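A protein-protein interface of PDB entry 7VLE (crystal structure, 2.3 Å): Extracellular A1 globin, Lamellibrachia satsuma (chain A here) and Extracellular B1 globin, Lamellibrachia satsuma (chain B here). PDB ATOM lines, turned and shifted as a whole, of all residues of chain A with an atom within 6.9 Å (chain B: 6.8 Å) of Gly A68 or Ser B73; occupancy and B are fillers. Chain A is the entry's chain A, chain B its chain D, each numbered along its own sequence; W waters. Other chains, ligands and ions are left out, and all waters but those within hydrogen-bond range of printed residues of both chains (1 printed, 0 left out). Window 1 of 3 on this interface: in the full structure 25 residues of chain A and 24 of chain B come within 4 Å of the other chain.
Water W1 bridges OG of Ser B73 (2.9 Å) and NH1 of Arg A72 (2.9 Å).
NH1 of Arg A24 is in salt-bridge range of OD1 of Asp B76, 2.6 Å away. The side-chain sulfur (SD) of Met B77 is in hydrogen-bond range of the backbone NH (N) of Arg A65, at 3.6 Å. The backbone carbonyl oxygen (O) of Gly A68 lies within hydrogen-bond range of the side-chain hydroxyl (OG) of Ser B73 (3.5 Å). The side-chain carboxylate (OD2) of Asp A71 is in salt-bridge range of the guanidinium group (NH2) of Arg B29 (2.9 Å). O of Ala A64 sits close to SD of Met B77 (3.7 Å).
The side-chain carboxylate of Asp A71 is in hydrogen-bond range of the indole nitrogen of Trp A14 (3.0 Å). The guanidinium group (NE) of Arg A24 sits close to the side-chain hydroxyl (OH) of Tyr A18 (3.4 Å). NE1 of Trp B16 sits at hydrogen-bond distance from OD2 of Asp B76 (2.4 Å). OH of Tyr B20 lies within hydrogen-bond range of NH2 of Arg B29, 3.3 Å away.
Among the printed residues, pairs that only touch across the chains: Arg A72 with Val B69 (3.7 Å) and Arg A72 with Arg B70 (3.7 Å).
Hydrophobic or aromatic side chains of chain A within 4 Å of the printed part of chain B: Ala A64. Hydrophobic or aromatic side chains of chain B that line the printed part of chain A: Val B69 and Met B77. Among the printed residues, 7 pairs touch across the chains. Among the printed residues, Asp or Glu carboxylates within 4 Å of a Lys or Arg side-chain nitrogen of the other chain: Arg A24 with Asp B76 (2.6 Å) and Asp A71 with Arg B29 (2.9 Å).
Printed residues of chain B within 4 Å of Arg A24: Asp B76 (2.6 Å). Of the printed residues of chain B, Arg A65 touches Met B77 (3.6 Å). Ile A67 touches none of the printed residues of chain B. Gly A68 touches just one residue of chain B: Ser B73. Of the printed residues of chain A, Val B69 touches Arg A72. Of chain A, only Gly A68 comes within 4 Å of Ser B73. Of the printed residues of chain A, Asp B76 touches Arg A24 (2.6 Å). Of the printed residues of chain A, Met B77 touches Ala A64 (3.6 Å) and Arg A65 (3.6 Å). The nearest residue of chain A that does not touch Ser B73 is Arg A72 (4.1 Å).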
ATOM      1  N   TRP A  14     -18.590  25.294 -32.170  1.00  0.00           N
ATOM      2  CA  TRP A  14     -18.878  25.304 -30.740  1.00  0.00           C
ATOM      3  C   TRP A  14     -17.594  25.357 -29.926  1.00  0.00           C
ATOM      4  O   TRP A  14     -17.455  26.189 -29.023  1.00  0.00           O
ATOM      5  CB  TRP A  14     -19.700  24.077 -30.350  1.00  0.00           C
ATOM      6  CG  TRP A  14     -19.700  23.826 -28.875  1.00  0.00           C
ATOM      7  CD1 TRP A  14     -19.009  22.857 -28.206  1.00  0.00           C
ATOM      8  CD2 TRP A  14     -20.412  24.571 -27.882  1.00  0.00           C
ATOM      9  NE1 TRP A  14     -19.255  22.948 -26.858  1.00  0.00           N
ATOM     10  CE2 TRP A  14     -20.113  23.992 -26.633  1.00  0.00           C
ATOM     11  CE3 TRP A  14     -21.276  25.668 -27.928  1.00  0.00           C
ATOM     12  CZ2 TRP A  14     -20.650  24.472 -25.442  1.00  0.00           C
ATOM     13  CZ3 TRP A  14     -21.806  26.145 -26.745  1.00  0.00           C
ATOM     14  CH2 TRP A  14     -21.491  25.548 -25.518  1.00  0.00           C
ATOM     15  N   TYR A  18     -16.760  28.478 -27.493  1.00  0.00           N
ATOM     16  CA  TYR A  18     -16.918  28.087 -26.096  1.00  0.00           C
ATOM     17  C   TYR A  18     -15.644  28.344 -25.299  1.00  0.00           C
ATOM     18  O   TYR A  18     -15.708  28.785 -24.145  1.00  0.00           O
ATOM     19  CB  TYR A  18     -17.315  26.613 -26.043  1.00  0.00           C
ATOM     20  CG  TYR A  18     -17.653  26.039 -24.694  1.00  0.00           C
ATOM     21  CD1 TYR A  18     -18.626  26.613 -23.888  1.00  0.00           C
ATOM     22  CD2 TYR A  18     -17.035  24.878 -24.253  1.00  0.00           C
ATOM     23  CE1 TYR A  18     -18.950  26.059 -22.665  1.00  0.00           C
ATOM     24  CE2 TYR A  18     -17.349  24.320 -23.037  1.00  0.00           C
ATOM     25  CZ  TYR A  18     -18.307  24.912 -22.246  1.00  0.00           C
ATOM     26  OH  TYR A  18     -18.620  24.348 -21.031  1.00  0.00           O
ATOM     27  N   ARG A  24     -15.540  30.542 -20.698  1.00  0.00           N
ATOM     28  CA  ARG A  24     -16.693  29.653 -20.670  1.00  0.00           C
ATOM     29  C   ARG A  24     -17.842  30.251 -19.864  1.00  0.00           C
ATOM     30  O   ARG A  24     -19.001  30.216 -20.298  1.00  0.00           O
ATOM     31  CB  ARG A  24     -16.234  28.318 -20.087  1.00  0.00           C
ATOM     32  CG  ARG A  24     -17.260  27.249 -19.896  1.00  0.00           C
ATOM     33  CD  ARG A  24     -16.534  25.965 -19.526  1.00  0.00           C
ATOM     34  NE  ARG A  24     -15.549  25.600 -20.542  1.00  0.00           N
ATOM     35  CZ  ARG A  24     -14.890  24.446 -20.566  1.00  0.00           C
ATOM     36  NH1 ARG A  24     -15.111  23.535 -19.628  1.00  0.00           N
ATOM     37  NH2 ARG A  24     -14.011  24.199 -21.528  1.00  0.00           N
ATOM     38  N   HIS A  62     -25.915  27.054 -12.109  1.00  0.00           N
ATOM     39  CA  HIS A  62     -26.889  26.585 -13.088  1.00  0.00           C
ATOM     40  C   HIS A  62     -26.385  26.794 -14.508  1.00  0.00           C
ATOM     41  O   HIS A  62     -26.504  25.903 -15.357  1.00  0.00           O
ATOM     42  CB  HIS A  62     -28.219  27.306 -12.884  1.00  0.00           C
ATOM     43  CG  HIS A  62     -29.239  26.987 -13.929  1.00  0.00           C
ATOM     44  ND1 HIS A  62     -29.827  25.746 -14.038  1.00  0.00           N
ATOM     45  CD2 HIS A  62     -29.767  27.741 -14.921  1.00  0.00           C
ATOM     46  CE1 HIS A  62     -30.678  25.751 -15.047  1.00  0.00           C
ATOM     47  NE2 HIS A  62     -30.661  26.950 -15.600  1.00  0.00           N
ATOM     48  N   ILE A  63     -25.826  27.977 -14.782  1.00  0.00           N
ATOM     49  CA  ILE A  63     -25.256  28.273 -16.096  1.00  0.00           C
ATOM     50  C   ILE A  63     -24.220  27.224 -16.474  1.00  0.00           C
ATOM     51  O   ILE A  63     -24.203  26.713 -17.602  1.00  0.00           O
ATOM     52  CB  ILE A  63     -24.640  29.683 -16.098  1.00  0.00           C
ATOM     53  CG1 ILE A  63     -25.731  30.755 -16.058  1.00  0.00           C
ATOM     54  CG2 ILE A  63     -23.718  29.863 -17.292  1.00  0.00           C
ATOM     55  CD1 ILE A  63     -25.187  32.169 -16.063  1.00  0.00           C
ATOM     56  N   ALA A  64     -23.336  26.894 -15.531  1.00  0.00           N
ATOM     57  CA  ALA A  64     -22.261  25.945 -15.802  1.00  0.00           C
ATOM     58  C   ALA A  64     -22.815  24.575 -16.169  1.00  0.00           C
ATOM     59  O   ALA A  64     -22.352  23.940 -17.123  1.00  0.00           O
ATOM     60  CB  ALA A  64     -21.338  25.845 -14.587  1.00  0.00           C
ATOM     61  N   ARG A  65     -23.807  24.100 -15.413  1.00  0.00           N
ATOM     62  CA  ARG A  65     -24.400  22.799 -15.701  1.00  0.00           C
ATOM     63  C   ARG A  65     -25.037  22.778 -17.085  1.00  0.00           C
ATOM     64  O   ARG A  65     -24.880  21.807 -17.834  1.00  0.00           O
ATOM     65  CB  ARG A  65     -25.432  22.440 -14.629  1.00  0.00           C
ATOM     66  CG  ARG A  65     -24.832  22.034 -13.292  1.00  0.00           C
ATOM     67  CD  ARG A  65     -25.890  21.463 -12.355  1.00  0.00           C
ATOM     68  NE  ARG A  65     -26.799  22.487 -11.849  1.00  0.00           N
ATOM     69  CZ  ARG A  65     -26.589  23.188 -10.739  1.00  0.00           C
ATOM     70  NH1 ARG A  65     -25.494  22.981 -10.020  1.00  0.00           N
ATOM     71  NH2 ARG A  65     -27.469  24.100 -10.349  1.00  0.00           N
ATOM     72  N   VAL A  66     -25.745  23.851 -17.446  1.00  0.00           N
ATOM     73  CA  VAL A  66     -26.442  23.897 -18.728  1.00  0.00           C
ATOM     74  C   VAL A  66     -25.449  23.882 -19.884  1.00  0.00           C
ATOM     75  O   VAL A  66     -25.555  23.058 -20.800  1.00  0.00           O
ATOM     76  CB  VAL A  66     -27.358  25.133 -18.797  1.00  0.00           C
ATOM     77  CG1 VAL A  66     -27.965  25.259 -20.184  1.00  0.00           C
ATOM     78  CG2 VAL A  66     -28.445  25.053 -17.739  1.00  0.00           C
ATOM     79  N   ILE A  67     -24.479  24.801 -19.870  1.00  0.00           N
ATOM     80  CA  ILE A  67     -23.517  24.862 -20.969  1.00  0.00           C
ATOM     81  C   ILE A  67     -22.619  23.636 -20.964  1.00  0.00           C
ATOM     82  O   ILE A  67     -22.143  23.203 -22.021  1.00  0.00           O
ATOM     83  CB  ILE A  67     -22.686  26.158 -20.916  1.00  0.00           C
ATOM     84  CG1 ILE A  67     -21.792  26.183 -19.674  1.00  0.00           C
ATOM     85  CG2 ILE A  67     -23.590  27.380 -20.970  1.00  0.00           C
ATOM     86  CD1 ILE A  67     -20.918  27.413 -19.576  1.00  0.00           C
ATOM     87  N   GLY A  68     -22.354  23.066 -19.788  1.00  0.00           N
ATOM     88  CA  GLY A  68     -21.701  21.773 -19.748  1.00  0.00           C
ATOM     89  C   GLY A  68     -22.555  20.694 -20.376  1.00  0.00           C
ATOM     90  O   GLY A  68     -22.035  19.777 -21.018  1.00  0.00           O
ATOM     91  N   GLY A  69     -23.877  20.794 -20.214  1.00  0.00           N
ATOM     92  CA  GLY A  69     -24.770  19.867 -20.885  1.00  0.00           C
ATOM     93  C   GLY A  69     -24.737  20.018 -22.394  1.00  0.00           C
ATOM     94  O   GLY A  69     -24.683  19.024 -23.121  1.00  0.00           O
ATOM     95  N   LEU A  70     -24.773  21.261 -22.884  1.00  0.00           N
ATOM     96  CA  LEU A  70     -24.625  21.503 -24.316  1.00  0.00           C
ATOM     97  C   LEU A  70     -23.333  20.895 -24.844  1.00  0.00           C
ATOM     98  O   LEU A  70     -23.321  20.240 -25.892  1.00  0.00           O
ATOM     99  CB  LEU A  70     -24.649  23.006 -24.604  1.00  0.00           C
ATOM    100  CG  LEU A  70     -25.994  23.707 -24.763  1.00  0.00           C
ATOM    101  CD1 LEU A  70     -25.780  25.199 -24.957  1.00  0.00           C
ATOM    102  CD2 LEU A  70     -26.759  23.118 -25.934  1.00  0.00           C
ATOM    103  N   ASP A  71     -22.233  21.099 -24.116  1.00  0.00           N
ATOM    104  CA  ASP A  71     -20.926  20.658 -24.589  1.00  0.00           C
ATOM    105  C   ASP A  71     -20.862  19.142 -24.722  1.00  0.00           C
ATOM    106  O   ASP A  71     -20.360  18.616 -25.722  1.00  0.00           O
ATOM    107  CB  ASP A  71     -19.837  21.148 -23.641  1.00  0.00           C
ATOM    108  CG  ASP A  71     -18.478  20.596 -23.998  1.00  0.00           C
ATOM    109  OD1 ASP A  71     -17.834  21.169 -24.897  1.00  0.00           O
ATOM    110  OD2 ASP A  71     -18.064  19.582 -23.398  1.00  0.00           O
ATOM    111  N   ARG A  72     -21.349  18.421 -23.710  1.00  0.00           N
ATOM    112  CA  ARG A  72     -21.269  16.964 -23.749  1.00  0.00           C
ATOM    113  C   ARG A  72     -22.190  16.393 -24.820  1.00  0.00           C
ATOM    114  O   ARG A  72     -21.842  15.411 -25.486  1.00  0.00           O
ATOM    115  CB  ARG A  72     -21.591  16.378 -22.372  1.00  0.00           C
ATOM    116  CG  ARG A  72     -23.033  16.545 -21.902  1.00  0.00           C
ATOM    117  CD  ARG A  72     -23.231  15.904 -20.536  1.00  0.00           C
ATOM    118  NE  ARG A  72     -24.546  15.285 -20.396  1.00  0.00           N
ATOM    119  CZ  ARG A  72     -25.430  15.593 -19.453  1.00  0.00           C
ATOM    120  NH1 ARG A  72     -25.145  16.515 -18.543  1.00  0.00           N
ATOM    121  NH2 ARG A  72     -26.599  14.969 -19.412  1.00  0.00           N
ATOM    122  N   VAL A  73     -23.357  17.010 -25.016  1.00  0.00           N
ATOM    123  CA  VAL A  73     -24.287  16.559 -26.047  1.00  0.00           C
ATOM    124  C   VAL A  73     -23.708  16.815 -27.433  1.00  0.00           C
ATOM    125  O   VAL A  73     -23.764  15.953 -28.318  1.00  0.00           O
ATOM    126  CB  VAL A  73     -25.653  17.249 -25.873  1.00  0.00           C
ATOM    127  CG1 VAL A  73     -26.536  16.990 -27.081  1.00  0.00           C
ATOM    128  CG2 VAL A  73     -26.334  16.774 -24.599  1.00  0.00           C
ATOM    129  N   TRP B  16      -5.630  19.674 -18.022  1.00  0.00           N
ATOM    130  CA  TRP B  16      -6.906  19.012 -18.272  1.00  0.00           C
ATOM    131  C   TRP B  16      -7.424  19.282 -19.682  1.00  0.00           C
ATOM    132  O   TRP B  16      -7.932  18.368 -20.340  1.00  0.00           O
ATOM    133  CB  TRP B  16      -7.936  19.459 -17.235  1.00  0.00           C
ATOM    134  CG  TRP B  16      -9.307  18.931 -17.496  1.00  0.00           C
ATOM    135  CD1 TRP B  16     -10.393  19.640 -17.921  1.00  0.00           C
ATOM    136  CD2 TRP B  16      -9.743  17.573 -17.360  1.00  0.00           C
ATOM    137  NE1 TRP B  16     -11.478  18.809 -18.052  1.00  0.00           N
ATOM    138  CE2 TRP B  16     -11.106  17.535 -17.713  1.00  0.00           C
ATOM    139  CE3 TRP B  16      -9.114  16.387 -16.968  1.00  0.00           C
ATOM    140  CZ2 TRP B  16     -11.851  16.357 -17.689  1.00  0.00           C
ATOM    141  CZ3 TRP B  16      -9.854  15.218 -16.945  1.00  0.00           C
ATOM    142  CH2 TRP B  16     -11.208  15.212 -17.303  1.00  0.00           C
ATOM    143  N   TYR B  20      -8.864  16.961 -22.594  1.00  0.00           N
ATOM    144  CA  TYR B  20     -10.315  17.068 -22.537  1.00  0.00           C
ATOM    145  C   TYR B  20     -10.714  18.491 -22.885  1.00  0.00           C
ATOM    146  O   TYR B  20     -10.358  19.426 -22.165  1.00  0.00           O
ATOM    147  CB  TYR B  20     -10.835  16.692 -21.150  1.00  0.00           C
ATOM    148  CG  TYR B  20     -12.339  16.657 -21.067  1.00  0.00           C
ATOM    149  CD1 TYR B  20     -13.074  17.825 -20.924  1.00  0.00           C
ATOM    150  CD2 TYR B  20     -13.026  15.454 -21.135  1.00  0.00           C
ATOM    151  CE1 TYR B  20     -14.447  17.799 -20.860  1.00  0.00           C
ATOM    152  CE2 TYR B  20     -14.404  15.418 -21.064  1.00  0.00           C
ATOM    153  CZ  TYR B  20     -15.109  16.595 -20.924  1.00  0.00           C
ATOM    154  OH  TYR B  20     -16.481  16.574 -20.853  1.00  0.00           O
ATOM    155  N   ARG B  29     -13.554  10.400 -25.206  1.00  0.00           N
ATOM    156  CA  ARG B  29     -14.188  10.751 -23.939  1.00  0.00           C
ATOM    157  C   ARG B  29     -14.561   9.506 -23.147  1.00  0.00           C
ATOM    158  O   ARG B  29     -14.221   9.384 -21.966  1.00  0.00           O
ATOM    159  CB  ARG B  29     -15.423  11.618 -24.195  1.00  0.00           C
ATOM    160  CG  ARG B  29     -15.171  13.118 -24.166  1.00  0.00           C
ATOM    161  CD  ARG B  29     -16.415  13.880 -24.606  1.00  0.00           C
ATOM    162  NE  ARG B  29     -16.497  15.217 -24.021  1.00  0.00           N
ATOM    163  CZ  ARG B  29     -16.072  16.326 -24.616  1.00  0.00           C
ATOM    164  NH1 ARG B  29     -15.527  16.271 -25.824  1.00  0.00           N
ATOM    165  NH2 ARG B  29     -16.196  17.496 -24.003  1.00  0.00           N
ATOM    166  N   HIS B  67     -23.160   7.892 -19.421  1.00  0.00           N
ATOM    167  CA  HIS B  67     -22.906   8.120 -18.002  1.00  0.00           C
ATOM    168  C   HIS B  67     -21.492   8.635 -17.774  1.00  0.00           C
ATOM    169  O   HIS B  67     -21.291   9.656 -17.108  1.00  0.00           O
ATOM    170  CB  HIS B  67     -23.125   6.843 -17.195  1.00  0.00           C
ATOM    171  CG  HIS B  67     -22.611   6.938 -15.793  1.00  0.00           C
ATOM    172  ND1 HIS B  67     -23.214   7.725 -14.833  1.00  0.00           N
ATOM    173  CD2 HIS B  67     -21.535   6.377 -15.193  1.00  0.00           C
ATOM    174  CE1 HIS B  67     -22.542   7.629 -13.702  1.00  0.00           C
ATOM    175  NE2 HIS B  67     -21.517   6.817 -13.892  1.00  0.00           N
ATOM    176  N   THR B  68     -20.497   7.925 -18.308  1.00  0.00           N
ATOM    177  CA  THR B  68     -19.111   8.356 -18.156  1.00  0.00           C
ATOM    178  C   THR B  68     -18.899   9.740 -18.751  1.00  0.00           C
ATOM    179  O   THR B  68     -18.123  10.542 -18.215  1.00  0.00           O
ATOM    180  CB  THR B  68     -18.170   7.348 -18.815  1.00  0.00           C
ATOM    181  OG1 THR B  68     -18.377   7.363 -20.234  1.00  0.00           O
ATOM    182  CG2 THR B  68     -18.432   5.947 -18.288  1.00  0.00           C
ATOM    183  N   VAL B  69     -19.581  10.037 -19.860  1.00  0.00           N
ATOM    184  CA  VAL B  69     -19.449  11.348 -20.490  1.00  0.00           C
ATOM    185  C   VAL B  69     -19.922  12.446 -19.547  1.00  0.00           C
ATOM    186  O   VAL B  69     -19.271  13.490 -19.414  1.00  0.00           O
ATOM    187  CB  VAL B  69     -20.215  11.380 -21.826  1.00  0.00           C
ATOM    188  CG1 VAL B  69     -20.481  12.815 -22.252  1.00  0.00           C
ATOM    189  CG2 VAL B  69     -19.431  10.649 -22.905  1.00  0.00           C
ATOM    190  N   ARG B  70     -21.054  12.234 -18.873  1.00  0.00           N
ATOM    191  CA  ARG B  70     -21.556  13.262 -17.972  1.00  0.00           C
ATOM    192  C   ARG B  70     -20.796  13.298 -16.651  1.00  0.00           C
ATOM    193  O   ARG B  70     -20.794  14.337 -15.983  1.00  0.00           O
ATOM    194  CB  ARG B  70     -23.060  13.081 -17.729  1.00  0.00           C
ATOM    195  CG  ARG B  70     -23.467  11.883 -16.887  1.00  0.00           C
ATOM    196  CD  ARG B  70     -24.989  11.805 -16.759  1.00  0.00           C
ATOM    197  NE  ARG B  70     -25.646  11.628 -18.052  1.00  0.00           N
ATOM    198  CZ  ARG B  70     -26.147  10.475 -18.486  1.00  0.00           C
ATOM    199  NH1 ARG B  70     -26.076   9.390 -17.727  1.00  0.00           N
ATOM    200  NH2 ARG B  70     -26.724  10.407 -19.679  1.00  0.00           N
ATOM    201  N   VAL B  71     -20.136  12.202 -16.270  1.00  0.00           N
ATOM    202  CA  VAL B  71     -19.243  12.236 -15.115  1.00  0.00           C
ATOM    203  C   VAL B  71     -18.017  13.085 -15.418  1.00  0.00           C
ATOM    204  O   VAL B  71     -17.660  13.990 -14.654  1.00  0.00           O
ATOM    205  CB  VAL B  71     -18.837  10.810 -14.702  1.00  0.00           C
ATOM    206  CG1 VAL B  71     -17.733  10.863 -13.653  1.00  0.00           C
ATOM    207  CG2 VAL B  71     -20.037  10.042 -14.187  1.00  0.00           C
ATOM    208  N   LEU B  72     -17.345  12.791 -16.536  1.00  0.00           N
ATOM    209  CA  LEU B  72     -16.174  13.566 -16.929  1.00  0.00           C
ATOM    210  C   LEU B  72     -16.535  15.016 -17.210  1.00  0.00           C
ATOM    211  O   LEU B  72     -15.733  15.919 -16.946  1.00  0.00           O
ATOM    212  CB  LEU B  72     -15.524  12.931 -18.157  1.00  0.00           C
ATOM    213  CG  LEU B  72     -15.003  11.508 -17.971  1.00  0.00           C
ATOM    214  CD1 LEU B  72     -14.576  10.927 -19.301  1.00  0.00           C
ATOM    215  CD2 LEU B  72     -13.847  11.491 -16.988  1.00  0.00           C
ATOM    216  N   SER B  73     -17.735  15.255 -17.746  1.00  0.00           N
ATOM    217  CA  SER B  73     -18.203  16.621 -17.963  1.00  0.00           C
ATOM    218  C   SER B  73     -18.366  17.363 -16.643  1.00  0.00           C
ATOM    219  O   SER B  73     -18.025  18.547 -16.541  1.00  0.00           O
ATOM    220  CB  SER B  73     -19.521  16.601 -18.736  1.00  0.00           C
ATOM    221  OG  SER B  73     -20.061  17.903 -18.871  1.00  0.00           O
ATOM    222  N   GLY B  74     -18.897  16.687 -15.623  1.00  0.00           N
ATOM    223  CA  GLY B  74     -18.992  17.307 -14.311  1.00  0.00           C
ATOM    224  C   GLY B  74     -17.629  17.555 -13.696  1.00  0.00           C
ATOM    225  O   GLY B  74     -17.390  18.606 -13.093  1.00  0.00           O
ATOM    226  N   LEU B  75     -16.718  16.588 -13.835  1.00  0.00           N
ATOM    227  CA  LEU B  75     -15.341  16.787 -13.397  1.00  0.00           C
ATOM    228  C   LEU B  75     -14.695  17.950 -14.135  1.00  0.00           C
ATOM    229  O   LEU B  75     -13.964  18.750 -13.538  1.00  0.00           O
ATOM    230  CB  LEU B  75     -14.541  15.500 -13.610  1.00  0.00           C
ATOM    231  CG  LEU B  75     -13.031  15.553 -13.382  1.00  0.00           C
ATOM    232  CD1 LEU B  75     -12.721  16.017 -11.971  1.00  0.00           C
ATOM    233  CD2 LEU B  75     -12.402  14.195 -13.651  1.00  0.00           C
ATOM    234  N   ASP B  76     -14.955  18.059 -15.440  1.00  0.00           N
ATOM    235  CA  ASP B  76     -14.451  19.187 -16.216  1.00  0.00           C
ATOM    236  C   ASP B  76     -15.026  20.500 -15.710  1.00  0.00           C
ATOM    237  O   ASP B  76     -14.319  21.511 -15.624  1.00  0.00           O
ATOM    238  CB  ASP B  76     -14.796  18.986 -17.690  1.00  0.00           C
ATOM    239  CG  ASP B  76     -14.404  20.166 -18.548  1.00  0.00           C
ATOM    240  OD1 ASP B  76     -15.267  21.029 -18.819  1.00  0.00           O
ATOM    241  OD2 ASP B  76     -13.223  20.236 -18.943  1.00  0.00           O
ATOM    242  N   MET B  77     -16.316  20.495 -15.371  1.00  0.00           N
ATOM    243  CA  MET B  77     -16.977  21.695 -14.874  1.00  0.00           C
ATOM    244  C   MET B  77     -16.359  22.167 -13.564  1.00  0.00           C
ATOM    245  O   MET B  77     -16.140  23.368 -13.369  1.00  0.00           O
ATOM    246  CB  MET B  77     -18.466  21.406 -14.704  1.00  0.00           C
ATOM    247  CG  MET B  77     -19.287  22.544 -14.150  1.00  0.00           C
ATOM    248  SD  MET B  77     -21.035  22.107 -14.165  1.00  0.00           S
ATOM    249  CE  MET B  77     -21.007  20.561 -13.259  1.00  0.00           C
ATOM    250  N   GLY B  78     -16.072  21.236 -12.653  1.00  0.00           N
ATOM    251  CA  GLY B  78     -15.421  21.617 -11.411  1.00  0.00           C
ATOM    252  C   GLY B  78     -14.025  22.163 -11.632  1.00  0.00           C
ATOM    253  O   GLY B  78     -13.637  23.166 -11.028  1.00  0.00           O
HETATM  254  O   HOH W   1     -22.733  17.991 -17.869  1.00  0.00           O
